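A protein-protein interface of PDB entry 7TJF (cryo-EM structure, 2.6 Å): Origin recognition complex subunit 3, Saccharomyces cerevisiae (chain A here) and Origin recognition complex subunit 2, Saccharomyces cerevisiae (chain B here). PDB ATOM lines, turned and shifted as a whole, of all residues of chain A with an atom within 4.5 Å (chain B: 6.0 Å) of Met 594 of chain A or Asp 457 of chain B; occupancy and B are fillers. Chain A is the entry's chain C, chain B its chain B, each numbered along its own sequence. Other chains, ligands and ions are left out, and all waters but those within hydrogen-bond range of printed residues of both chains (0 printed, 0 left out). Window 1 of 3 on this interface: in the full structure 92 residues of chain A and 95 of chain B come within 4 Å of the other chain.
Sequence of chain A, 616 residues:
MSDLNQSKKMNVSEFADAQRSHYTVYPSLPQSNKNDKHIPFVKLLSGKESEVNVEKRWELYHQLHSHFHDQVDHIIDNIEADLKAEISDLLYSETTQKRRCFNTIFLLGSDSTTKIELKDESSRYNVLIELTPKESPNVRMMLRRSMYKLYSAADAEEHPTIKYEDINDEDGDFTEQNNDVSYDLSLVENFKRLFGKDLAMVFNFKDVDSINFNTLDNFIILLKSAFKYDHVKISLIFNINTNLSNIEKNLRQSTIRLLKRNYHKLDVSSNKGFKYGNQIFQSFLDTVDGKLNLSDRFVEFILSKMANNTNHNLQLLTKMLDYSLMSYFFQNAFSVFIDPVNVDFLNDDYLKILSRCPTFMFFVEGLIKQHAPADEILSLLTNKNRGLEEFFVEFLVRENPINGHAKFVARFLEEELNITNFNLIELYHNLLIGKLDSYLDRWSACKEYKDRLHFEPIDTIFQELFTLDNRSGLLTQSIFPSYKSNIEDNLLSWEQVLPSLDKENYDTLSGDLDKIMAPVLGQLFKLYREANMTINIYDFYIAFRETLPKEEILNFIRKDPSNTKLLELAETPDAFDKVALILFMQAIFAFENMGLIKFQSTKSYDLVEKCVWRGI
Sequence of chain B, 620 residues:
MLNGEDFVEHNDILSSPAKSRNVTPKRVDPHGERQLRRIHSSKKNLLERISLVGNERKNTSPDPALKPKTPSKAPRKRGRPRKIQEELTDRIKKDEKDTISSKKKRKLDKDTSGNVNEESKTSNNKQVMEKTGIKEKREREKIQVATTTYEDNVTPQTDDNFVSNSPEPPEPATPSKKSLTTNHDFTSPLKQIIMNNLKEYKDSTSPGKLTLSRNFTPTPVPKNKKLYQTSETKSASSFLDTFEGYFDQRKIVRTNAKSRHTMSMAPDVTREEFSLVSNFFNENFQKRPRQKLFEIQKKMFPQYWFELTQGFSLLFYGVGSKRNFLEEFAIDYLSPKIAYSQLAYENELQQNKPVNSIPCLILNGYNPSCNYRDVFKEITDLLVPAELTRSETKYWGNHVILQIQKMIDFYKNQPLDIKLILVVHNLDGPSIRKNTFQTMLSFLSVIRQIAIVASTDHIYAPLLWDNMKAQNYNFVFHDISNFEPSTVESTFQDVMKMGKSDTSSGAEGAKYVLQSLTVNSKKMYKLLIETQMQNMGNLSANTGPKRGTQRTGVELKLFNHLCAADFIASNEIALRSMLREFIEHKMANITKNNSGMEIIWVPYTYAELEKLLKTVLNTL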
ATOM      1  N   ILE A 487      18.447  19.998  11.745  1.00  0.00           N
ATOM      2  CA  ILE A 487      19.028  19.756  13.068  1.00  0.00           C
ATOM      3  C   ILE A 487      19.434  21.072  13.730  1.00  0.00           C
ATOM      4  O   ILE A 487      19.145  21.301  14.914  1.00  0.00           O
ATOM      5  CB  ILE A 487      20.220  18.784  12.964  1.00  0.00           C
ATOM      6  CG1 ILE A 487      19.764  17.431  12.422  1.00  0.00           C
ATOM      7  CG2 ILE A 487      20.888  18.595  14.322  1.00  0.00           C
ATOM      8  CD1 ILE A 487      18.780  16.734  13.302  1.00  0.00           C
ATOM      9  N   LEU A 491      17.708  22.759  17.041  1.00  0.00           N
ATOM     10  CA  LEU A 491      18.526  23.072  18.209  1.00  0.00           C
ATOM     11  C   LEU A 491      18.399  24.538  18.609  1.00  0.00           C
ATOM     12  O   LEU A 491      18.283  24.851  19.798  1.00  0.00           O
ATOM     13  CB  LEU A 491      19.988  22.727  17.933  1.00  0.00           C
ATOM     14  CG  LEU A 491      20.374  21.268  18.153  1.00  0.00           C
ATOM     15  CD1 LEU A 491      21.754  20.990  17.575  1.00  0.00           C
ATOM     16  CD2 LEU A 491      20.316  20.931  19.633  1.00  0.00           C
ATOM     17  N   ALA A 590      26.574  14.885  24.481  1.00  0.00           N
ATOM     18  CA  ALA A 590      25.585  14.782  23.409  1.00  0.00           C
ATOM     19  C   ALA A 590      26.032  15.547  22.163  1.00  0.00           C
ATOM     20  O   ALA A 590      25.875  15.058  21.035  1.00  0.00           O
ATOM     21  CB  ALA A 590      24.229  15.284  23.898  1.00  0.00           C
ATOM     22  N   PHE A 591      26.607  16.742  22.355  1.00  0.00           N
ATOM     23  CA  PHE A 591      27.163  17.519  21.248  1.00  0.00           C
ATOM     24  C   PHE A 591      28.317  16.785  20.578  1.00  0.00           C
ATOM     25  O   PHE A 591      28.450  16.811  19.348  1.00  0.00           O
ATOM     26  CB  PHE A 591      27.644  18.880  21.752  1.00  0.00           C
ATOM     27  CG  PHE A 591      26.639  19.986  21.605  1.00  0.00           C
ATOM     28  CD1 PHE A 591      25.286  19.747  21.792  1.00  0.00           C
ATOM     29  CD2 PHE A 591      27.054  21.274  21.304  1.00  0.00           C
ATOM     30  CE1 PHE A 591      24.364  20.771  21.668  1.00  0.00           C
ATOM     31  CE2 PHE A 591      26.138  22.304  21.178  1.00  0.00           C
ATOM     32  CZ  PHE A 591      24.790  22.050  21.361  1.00  0.00           C
ATOM     33  N   GLU A 592      29.166  16.135  21.378  1.00  0.00           N
ATOM     34  CA  GLU A 592      30.312  15.401  20.849  1.00  0.00           C
ATOM     35  C   GLU A 592      29.860  14.180  20.054  1.00  0.00           C
ATOM     36  O   GLU A 592      30.468  13.841  19.033  1.00  0.00           O
ATOM     37  CB  GLU A 592      31.242  15.017  22.009  1.00  0.00           C
ATOM     38  CG  GLU A 592      32.677  14.544  21.678  1.00  0.00           C
ATOM     39  CD  GLU A 592      32.768  13.160  21.056  1.00  0.00           C
ATOM     40  OE1 GLU A 592      32.106  12.231  21.566  1.00  0.00           O
ATOM     41  OE2 GLU A 592      33.498  13.004  20.056  1.00  0.00           O
ATOM     42  N   ASN A 593      28.797  13.509  20.502  1.00  0.00           N
ATOM     43  CA  ASN A 593      28.289  12.374  19.743  1.00  0.00           C
ATOM     44  C   ASN A 593      27.575  12.810  18.468  1.00  0.00           C
ATOM     45  O   ASN A 593      27.616  12.089  17.466  1.00  0.00           O
ATOM     46  CB  ASN A 593      27.357  11.527  20.604  1.00  0.00           C
ATOM     47  CG  ASN A 593      27.175  10.131  20.050  1.00  0.00           C
ATOM     48  OD1 ASN A 593      28.052   9.280  20.187  1.00  0.00           O
ATOM     49  ND2 ASN A 593      26.041   9.892  19.405  1.00  0.00           N
ATOM     50  N   MET A 594      26.916  13.975  18.482  1.00  0.00           N
ATOM     51  CA  MET A 594      26.262  14.467  17.272  1.00  0.00           C
ATOM     52  C   MET A 594      27.255  14.934  16.210  1.00  0.00           C
ATOM     53  O   MET A 594      26.896  14.994  15.031  1.00  0.00           O
ATOM     54  CB  MET A 594      25.308  15.612  17.611  1.00  0.00           C
ATOM     55  CG  MET A 594      24.026  15.184  18.304  1.00  0.00           C
ATOM     56  SD  MET A 594      23.101  16.586  18.954  1.00  0.00           S
ATOM     57  CE  MET A 594      22.077  16.991  17.544  1.00  0.00           C
ATOM     58  N   GLY A 595      28.486  15.257  16.593  1.00  0.00           N
ATOM     59  CA  GLY A 595      29.459  15.804  15.674  1.00  0.00           C
ATOM     60  C   GLY A 595      29.554  17.311  15.665  1.00  0.00           C
ATOM     61  O   GLY A 595      30.198  17.867  14.769  1.00  0.00           O
ATOM     62  N   LEU A 596      28.928  17.989  16.628  1.00  0.00           N
ATOM     63  CA  LEU A 596      28.929  19.447  16.643  1.00  0.00           C
ATOM     64  C   LEU A 596      30.269  20.003  17.111  1.00  0.00           C
ATOM     65  O   LEU A 596      30.757  20.998  16.563  1.00  0.00           O
ATOM     66  CB  LEU A 596      27.793  19.959  17.528  1.00  0.00           C
ATOM     67  CG  LEU A 596      26.530  20.416  16.796  1.00  0.00           C
ATOM     68  CD1 LEU A 596      25.778  19.231  16.219  1.00  0.00           C
ATOM     69  CD2 LEU A 596      25.636  21.211  17.723  1.00  0.00           C
ATOM     70  N   PHE B 316      14.739   7.922  10.428  1.00  0.00           N
ATOM     71  CA  PHE B 316      14.354   8.899  11.428  1.00  0.00           C
ATOM     72  C   PHE B 316      15.584   9.658  11.895  1.00  0.00           C
ATOM     73  O   PHE B 316      16.671   9.092  12.012  1.00  0.00           O
ATOM     74  CB  PHE B 316      13.660   8.214  12.604  1.00  0.00           C
ATOM     75  CG  PHE B 316      12.342   7.606  12.245  1.00  0.00           C
ATOM     76  CD1 PHE B 316      11.204   8.390  12.171  1.00  0.00           C
ATOM     77  CD2 PHE B 316      12.243   6.254  11.951  1.00  0.00           C
ATOM     78  CE1 PHE B 316       9.992   7.836  11.830  1.00  0.00           C
ATOM     79  CE2 PHE B 316      11.027   5.694  11.610  1.00  0.00           C
ATOM     80  CZ  PHE B 316       9.901   6.488  11.548  1.00  0.00           C
ATOM     81  N   GLY B 318      16.739  13.551  14.225  1.00  0.00           N
ATOM     82  CA  GLY B 318      16.300  14.630  15.080  1.00  0.00           C
ATOM     83  C   GLY B 318      17.240  14.790  16.254  1.00  0.00           C
ATOM     84  O   GLY B 318      18.277  14.141  16.339  1.00  0.00           O
ATOM     85  N   VAL B 319      16.844  15.672  17.162  1.00  0.00           N
ATOM     86  CA  VAL B 319      17.596  15.949  18.377  1.00  0.00           C
ATOM     87  C   VAL B 319      17.003  15.109  19.498  1.00  0.00           C
ATOM     88  O   VAL B 319      15.824  15.259  19.840  1.00  0.00           O
ATOM     89  CB  VAL B 319      17.563  17.444  18.728  1.00  0.00           C
ATOM     90  CG1 VAL B 319      18.366  17.710  19.988  1.00  0.00           C
ATOM     91  CG2 VAL B 319      18.082  18.271  17.563  1.00  0.00           C
ATOM     92  N   GLY B 320      17.814  14.233  20.071  1.00  0.00           N
ATOM     93  CA  GLY B 320      17.396  13.381  21.164  1.00  0.00           C
ATOM     94  C   GLY B 320      17.368  11.913  20.766  1.00  0.00           C
ATOM     95  O   GLY B 320      17.545  11.541  19.606  1.00  0.00           O
ATOM     96  N   SER B 321      17.141  11.078  21.777  1.00  0.00           N
ATOM     97  CA  SER B 321      17.089   9.639  21.568  1.00  0.00           C
ATOM     98  C   SER B 321      15.840   9.252  20.795  1.00  0.00           C
ATOM     99  O   SER B 321      14.737   9.723  21.092  1.00  0.00           O
ATOM    100  CB  SER B 321      17.108   8.897  22.899  1.00  0.00           C
ATOM    101  OG  SER B 321      17.037   7.497  22.703  1.00  0.00           O
ATOM    102  N   LYS B 322      16.018   8.383  19.807  1.00  0.00           N
ATOM    103  CA  LYS B 322      14.919   7.855  19.020  1.00  0.00           C
ATOM    104  C   LYS B 322      14.737   6.359  19.233  1.00  0.00           C
ATOM    105  O   LYS B 322      14.018   5.714  18.464  1.00  0.00           O
ATOM    106  CB  LYS B 322      15.149   8.172  17.543  1.00  0.00           C
ATOM    107  CG  LYS B 322      15.392   9.654  17.286  1.00  0.00           C
ATOM    108  CD  LYS B 322      15.869   9.912  15.872  1.00  0.00           C
ATOM    109  CE  LYS B 322      17.357   9.729  15.770  1.00  0.00           C
ATOM    110  NZ  LYS B 322      18.088  10.707  16.621  1.00  0.00           N
ATOM    111  N   ASN B 426      20.655   3.840  15.467  1.00  0.00           N
ATOM    112  CA  ASN B 426      21.937   4.512  15.215  1.00  0.00           C
ATOM    113  C   ASN B 426      22.679   3.883  14.029  1.00  0.00           C
ATOM    114  O   ASN B 426      23.727   3.258  14.177  1.00  0.00           O
ATOM    115  CB  ASN B 426      22.816   4.519  16.474  1.00  0.00           C
ATOM    116  CG  ASN B 426      22.423   5.605  17.450  1.00  0.00           C
ATOM    117  OD1 ASN B 426      21.626   5.378  18.357  1.00  0.00           O
ATOM    118  ND2 ASN B 426      22.984   6.792  17.271  1.00  0.00           N
ATOM    119  N   LEU B 427      22.083   4.058  12.842  1.00  0.00           N
ATOM    120  CA  LEU B 427      22.665   3.574  11.590  1.00  0.00           C
ATOM    121  C   LEU B 427      24.010   4.233  11.270  1.00  0.00           C
ATOM    122  O   LEU B 427      24.801   3.675  10.502  1.00  0.00           O
ATOM    123  CB  LEU B 427      21.664   3.801  10.447  1.00  0.00           C
ATOM    124  CG  LEU B 427      21.958   3.366   9.005  1.00  0.00           C
ATOM    125  CD1 LEU B 427      22.034   1.860   8.896  1.00  0.00           C
ATOM    126  CD2 LEU B 427      20.936   3.927   8.033  1.00  0.00           C
ATOM    127  N   ASP B 428      24.295   5.396  11.850  1.00  0.00           N
ATOM    128  CA  ASP B 428      25.585   6.055  11.724  1.00  0.00           C
ATOM    129  C   ASP B 428      26.488   5.804  12.928  1.00  0.00           C
ATOM    130  O   ASP B 428      27.376   6.614  13.207  1.00  0.00           O
ATOM    131  CB  ASP B 428      25.371   7.552  11.520  1.00  0.00           C
ATOM    132  CG  ASP B 428      24.368   8.127  12.495  1.00  0.00           C
ATOM    133  OD1 ASP B 428      23.806   7.354  13.299  1.00  0.00           O
ATOM    134  OD2 ASP B 428      24.121   9.345  12.448  1.00  0.00           O
ATOM    135  N   SER B 455      17.546   4.786  12.286  1.00  0.00           N
ATOM    136  CA  SER B 455      17.702   6.104  12.880  1.00  0.00           C
ATOM    137  C   SER B 455      19.159   6.530  12.782  1.00  0.00           C
ATOM    138  O   SER B 455      20.060   5.692  12.725  1.00  0.00           O
ATOM    139  CB  SER B 455      17.239   6.125  14.343  1.00  0.00           C
ATOM    140  OG  SER B 455      18.109   5.366  15.162  1.00  0.00           O
ATOM    141  N   THR B 456      19.383   7.842  12.744  1.00  0.00           N
ATOM    142  CA  THR B 456      20.724   8.404  12.654  1.00  0.00           C
ATOM    143  C   THR B 456      20.875   9.549  13.644  1.00  0.00           C
ATOM    144  O   THR B 456      19.937  10.312  13.879  1.00  0.00           O
ATOM    145  CB  THR B 456      21.046   8.924  11.240  1.00  0.00           C
ATOM    146  OG1 THR B 456      19.957   9.718  10.760  1.00  0.00           O
ATOM    147  CG2 THR B 456      21.310   7.773  10.277  1.00  0.00           C
ATOM    148  N   ASP B 457      22.078   9.676  14.203  1.00  0.00           N
ATOM    149  CA  ASP B 457      22.371  10.718  15.175  1.00  0.00           C
ATOM    150  C   ASP B 457      23.401  11.739  14.715  1.00  0.00           C
ATOM    151  O   ASP B 457      23.373  12.871  15.207  1.00  0.00           O
ATOM    152  CB  ASP B 457      22.861  10.101  16.494  1.00  0.00           C
ATOM    153  CG  ASP B 457      21.751   9.926  17.501  1.00  0.00           C
ATOM    154  OD1 ASP B 457      20.720  10.616  17.373  1.00  0.00           O
ATOM    155  OD2 ASP B 457      21.908   9.099  18.423  1.00  0.00           O
ATOM    156  N   HIS B 458      24.302  11.384  13.806  1.00  0.00           N
ATOM    157  CA  HIS B 458      25.351  12.305  13.396  1.00  0.00           C
ATOM    158  C   HIS B 458      24.815  13.345  12.422  1.00  0.00           C
ATOM    159  O   HIS B 458      23.934  13.071  11.603  1.00  0.00           O
ATOM    160  CB  HIS B 458      26.520  11.553  12.760  1.00  0.00           C
ATOM    161  CG  HIS B 458      27.839  12.237  12.928  1.00  0.00           C
ATOM    162  ND1 HIS B 458      28.308  13.176  12.035  1.00  0.00           N
ATOM    163  CD2 HIS B 458      28.791  12.119  13.883  1.00  0.00           C
ATOM    164  CE1 HIS B 458      29.490  13.608  12.434  1.00  0.00           C
ATOM    165  NE2 HIS B 458      29.806  12.983  13.553  1.00  0.00           N
ATOM    166  N   ILE B 459      25.373  14.553  12.513  1.00  0.00           N
ATOM    167  CA  ILE B 459      24.960  15.643  11.640  1.00  0.00           C
ATOM    168  C   ILE B 459      25.454  15.443  10.207  1.00  0.00           C
ATOM    169  O   ILE B 459      24.911  16.048   9.276  1.00  0.00           O
ATOM    170  CB  ILE B 459      25.434  16.984  12.245  1.00  0.00           C
ATOM    171  CG1 ILE B 459      24.587  18.151  11.735  1.00  0.00           C
ATOM    172  CG2 ILE B 459      26.920  17.226  11.987  1.00  0.00           C
ATOM    173  CD1 ILE B 459      24.238  19.153  12.789  1.00  0.00           C
ATOM    174  N   TYR B 460      26.447  14.577   9.994  1.00  0.00           N
ATOM    175  CA  TYR B 460      27.014  14.343   8.673  1.00  0.00           C
ATOM    176  C   TYR B 460      26.649  12.975   8.111  1.00  0.00           C
ATOM    177  O   TYR B 460      27.328  12.494   7.203  1.00  0.00           O
ATOM    178  CB  TYR B 460      28.535  14.497   8.712  1.00  0.00           C
ATOM    179  CG  TYR B 460      29.022  15.925   8.672  1.00  0.00           C
ATOM    180  CD1 TYR B 460      28.215  16.947   8.181  1.00  0.00           C
ATOM    181  CD2 TYR B 460      30.296  16.250   9.119  1.00  0.00           C
ATOM    182  CE1 TYR B 460      28.663  18.255   8.146  1.00  0.00           C
ATOM    183  CE2 TYR B 460      30.754  17.550   9.086  1.00  0.00           C
ATOM    184  CZ  TYR B 460      29.935  18.547   8.600  1.00  0.00           C
ATOM    185  OH  TYR B 460      30.396  19.841   8.568  1.00  0.00           O
ATOM    186  N   ALA B 461      25.605  12.339   8.645  1.00  0.00           N
ATOM    187  CA  ALA B 461      25.183  11.010   8.195  1.00  0.00           C
ATOM    188  C   ALA B 461      24.870  10.858   6.697  1.00  0.00           C
ATOM    189  O   ALA B 461      25.239   9.809   6.140  1.00  0.00           O
ATOM    190  CB  ALA B 461      23.991  10.543   9.049  1.00  0.00           C
ATOM    191  N   SER B 486      18.718  10.133  26.002  1.00  0.00           N
ATOM    192  CA  SER B 486      19.697   9.198  25.423  1.00  0.00           C
ATOM    193  C   SER B 486      20.665   8.660  26.482  1.00  0.00           C
ATOM    194  O   SER B 486      21.880   8.849  26.414  1.00  0.00           O
ATOM    195  CB  SER B 486      20.455   9.823  24.241  1.00  0.00           C
ATOM    196  OG  SER B 486      21.707   9.190  24.049  1.00  0.00           O
ATOM    197  N   GLU B 489      22.349   4.899  25.157  1.00  0.00           N
ATOM    198  CA  GLU B 489      23.481   5.040  24.249  1.00  0.00           C
ATOM    199  C   GLU B 489      24.705   5.649  24.924  1.00  0.00           C
ATOM    200  O   GLU B 489      25.811   5.533  24.389  1.00  0.00           O
ATOM    201  CB  GLU B 489      23.071   5.892  23.045  1.00  0.00           C
ATOM    202  CG  GLU B 489      21.814   5.409  22.333  1.00  0.00           C
ATOM    203  CD  GLU B 489      20.550   6.113  22.807  1.00  0.00           C
ATOM    204  OE1 GLU B 489      20.298   6.137  24.030  1.00  0.00           O
ATOM    205  OE2 GLU B 489      19.803   6.637  21.954  1.00  0.00           O
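The backbone NH (N) of Ile 459 of chain B is in hydrogen-bond range of the backbone carbonyl oxygen (O) of Met 594 of chain A, 3.0 Å away.
The backbone carbonyl oxygen of Phe 591 of chain A lies within hydrogen-bond range of the backbone NH of Leu 596 of chain A, at 3.0 Å. The side-chain carboxylate (OD2) of Asp 428 of chain B lies within hydrogen-bond range of the backbone NH (N) of His 458 of chain B (2.5 Å). ND1 of His 458 of chain B is in hydrogen-bond range of N of Tyr 460 of chain B (3.1 Å). The backbone NH (N) of Asp 457 of chain B lies within hydrogen-bond range of the side-chain carboxylate (OD2) of Asp 428 of chain B, 2.7 Å away. The backbone carbonyl oxygen (O) of Gly 318 of chain B lies within hydrogen-bond range of the side-chain amino group (NZ) of Lys 322 of chain B, at 3.5 Å. OD2 of Asp 457 of chain B is in hydrogen-bond range of ND2 of Asn 426 of chain B (2.8 Å).
Among the printed residues, merely in contact across the chains: Ile 487 of chain A with Gly 318 of chain B, Ile 487 of chain A with Ile 459 of chain B, Leu 491 of chain A with Val 319 of chain B, Asn 593 of chain A with His 458 of chain B, Met 594 of chain A with Asp 457 of chain B, Met 594 of chain A with His 458 of chain B, Gly 595 of chain A with His 458 of chain B and Leu 596 of chain A with Ile 459 of chain B.
Of the printed residues of chain B, Ile 487 of chain A touches Gly 318 (3.7 Å) and Ile 459 (3.7 Å). Printed residues of chain B within 4 Å of Leu 491 of chain A: Val 319 (3.8 Å). Of the printed residues of chain B, Gly 595 of chain A touches His 458. Printed residues of chain A within 4 Å of Val 319 of chain B: Leu 491 (3.8 Å). Of chain A, only Met 594 comes within 4 Å of Asp 457 of chain B. Printed residues of chain A within 4 Å of His 458 of chain B: Asn 593 (3.8 Å), Met 594 (3.5 Å) and Gly 595 (3.5 Å). Glu 489 of chain B touches none of the printed residues of chain A. The nearest residue of chain B that does not touch Met 594 of chain A is Val 319 of chain B (4.2 Å). The nearest residue of chain A that does not touch Asp 457 of chain B is Asn 593 of chain A (4.3 Å).
Of the 9 printed residues of chain A, 6 touch a printed residue of chain B. Hydrophobic or aromatic side chains of chain A that line the printed part of chain B: Ile 487, Leu 491, Met 594 and Leu 596. Of the 18 printed residues of chain B, 5 touch a printed residue of chain A.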
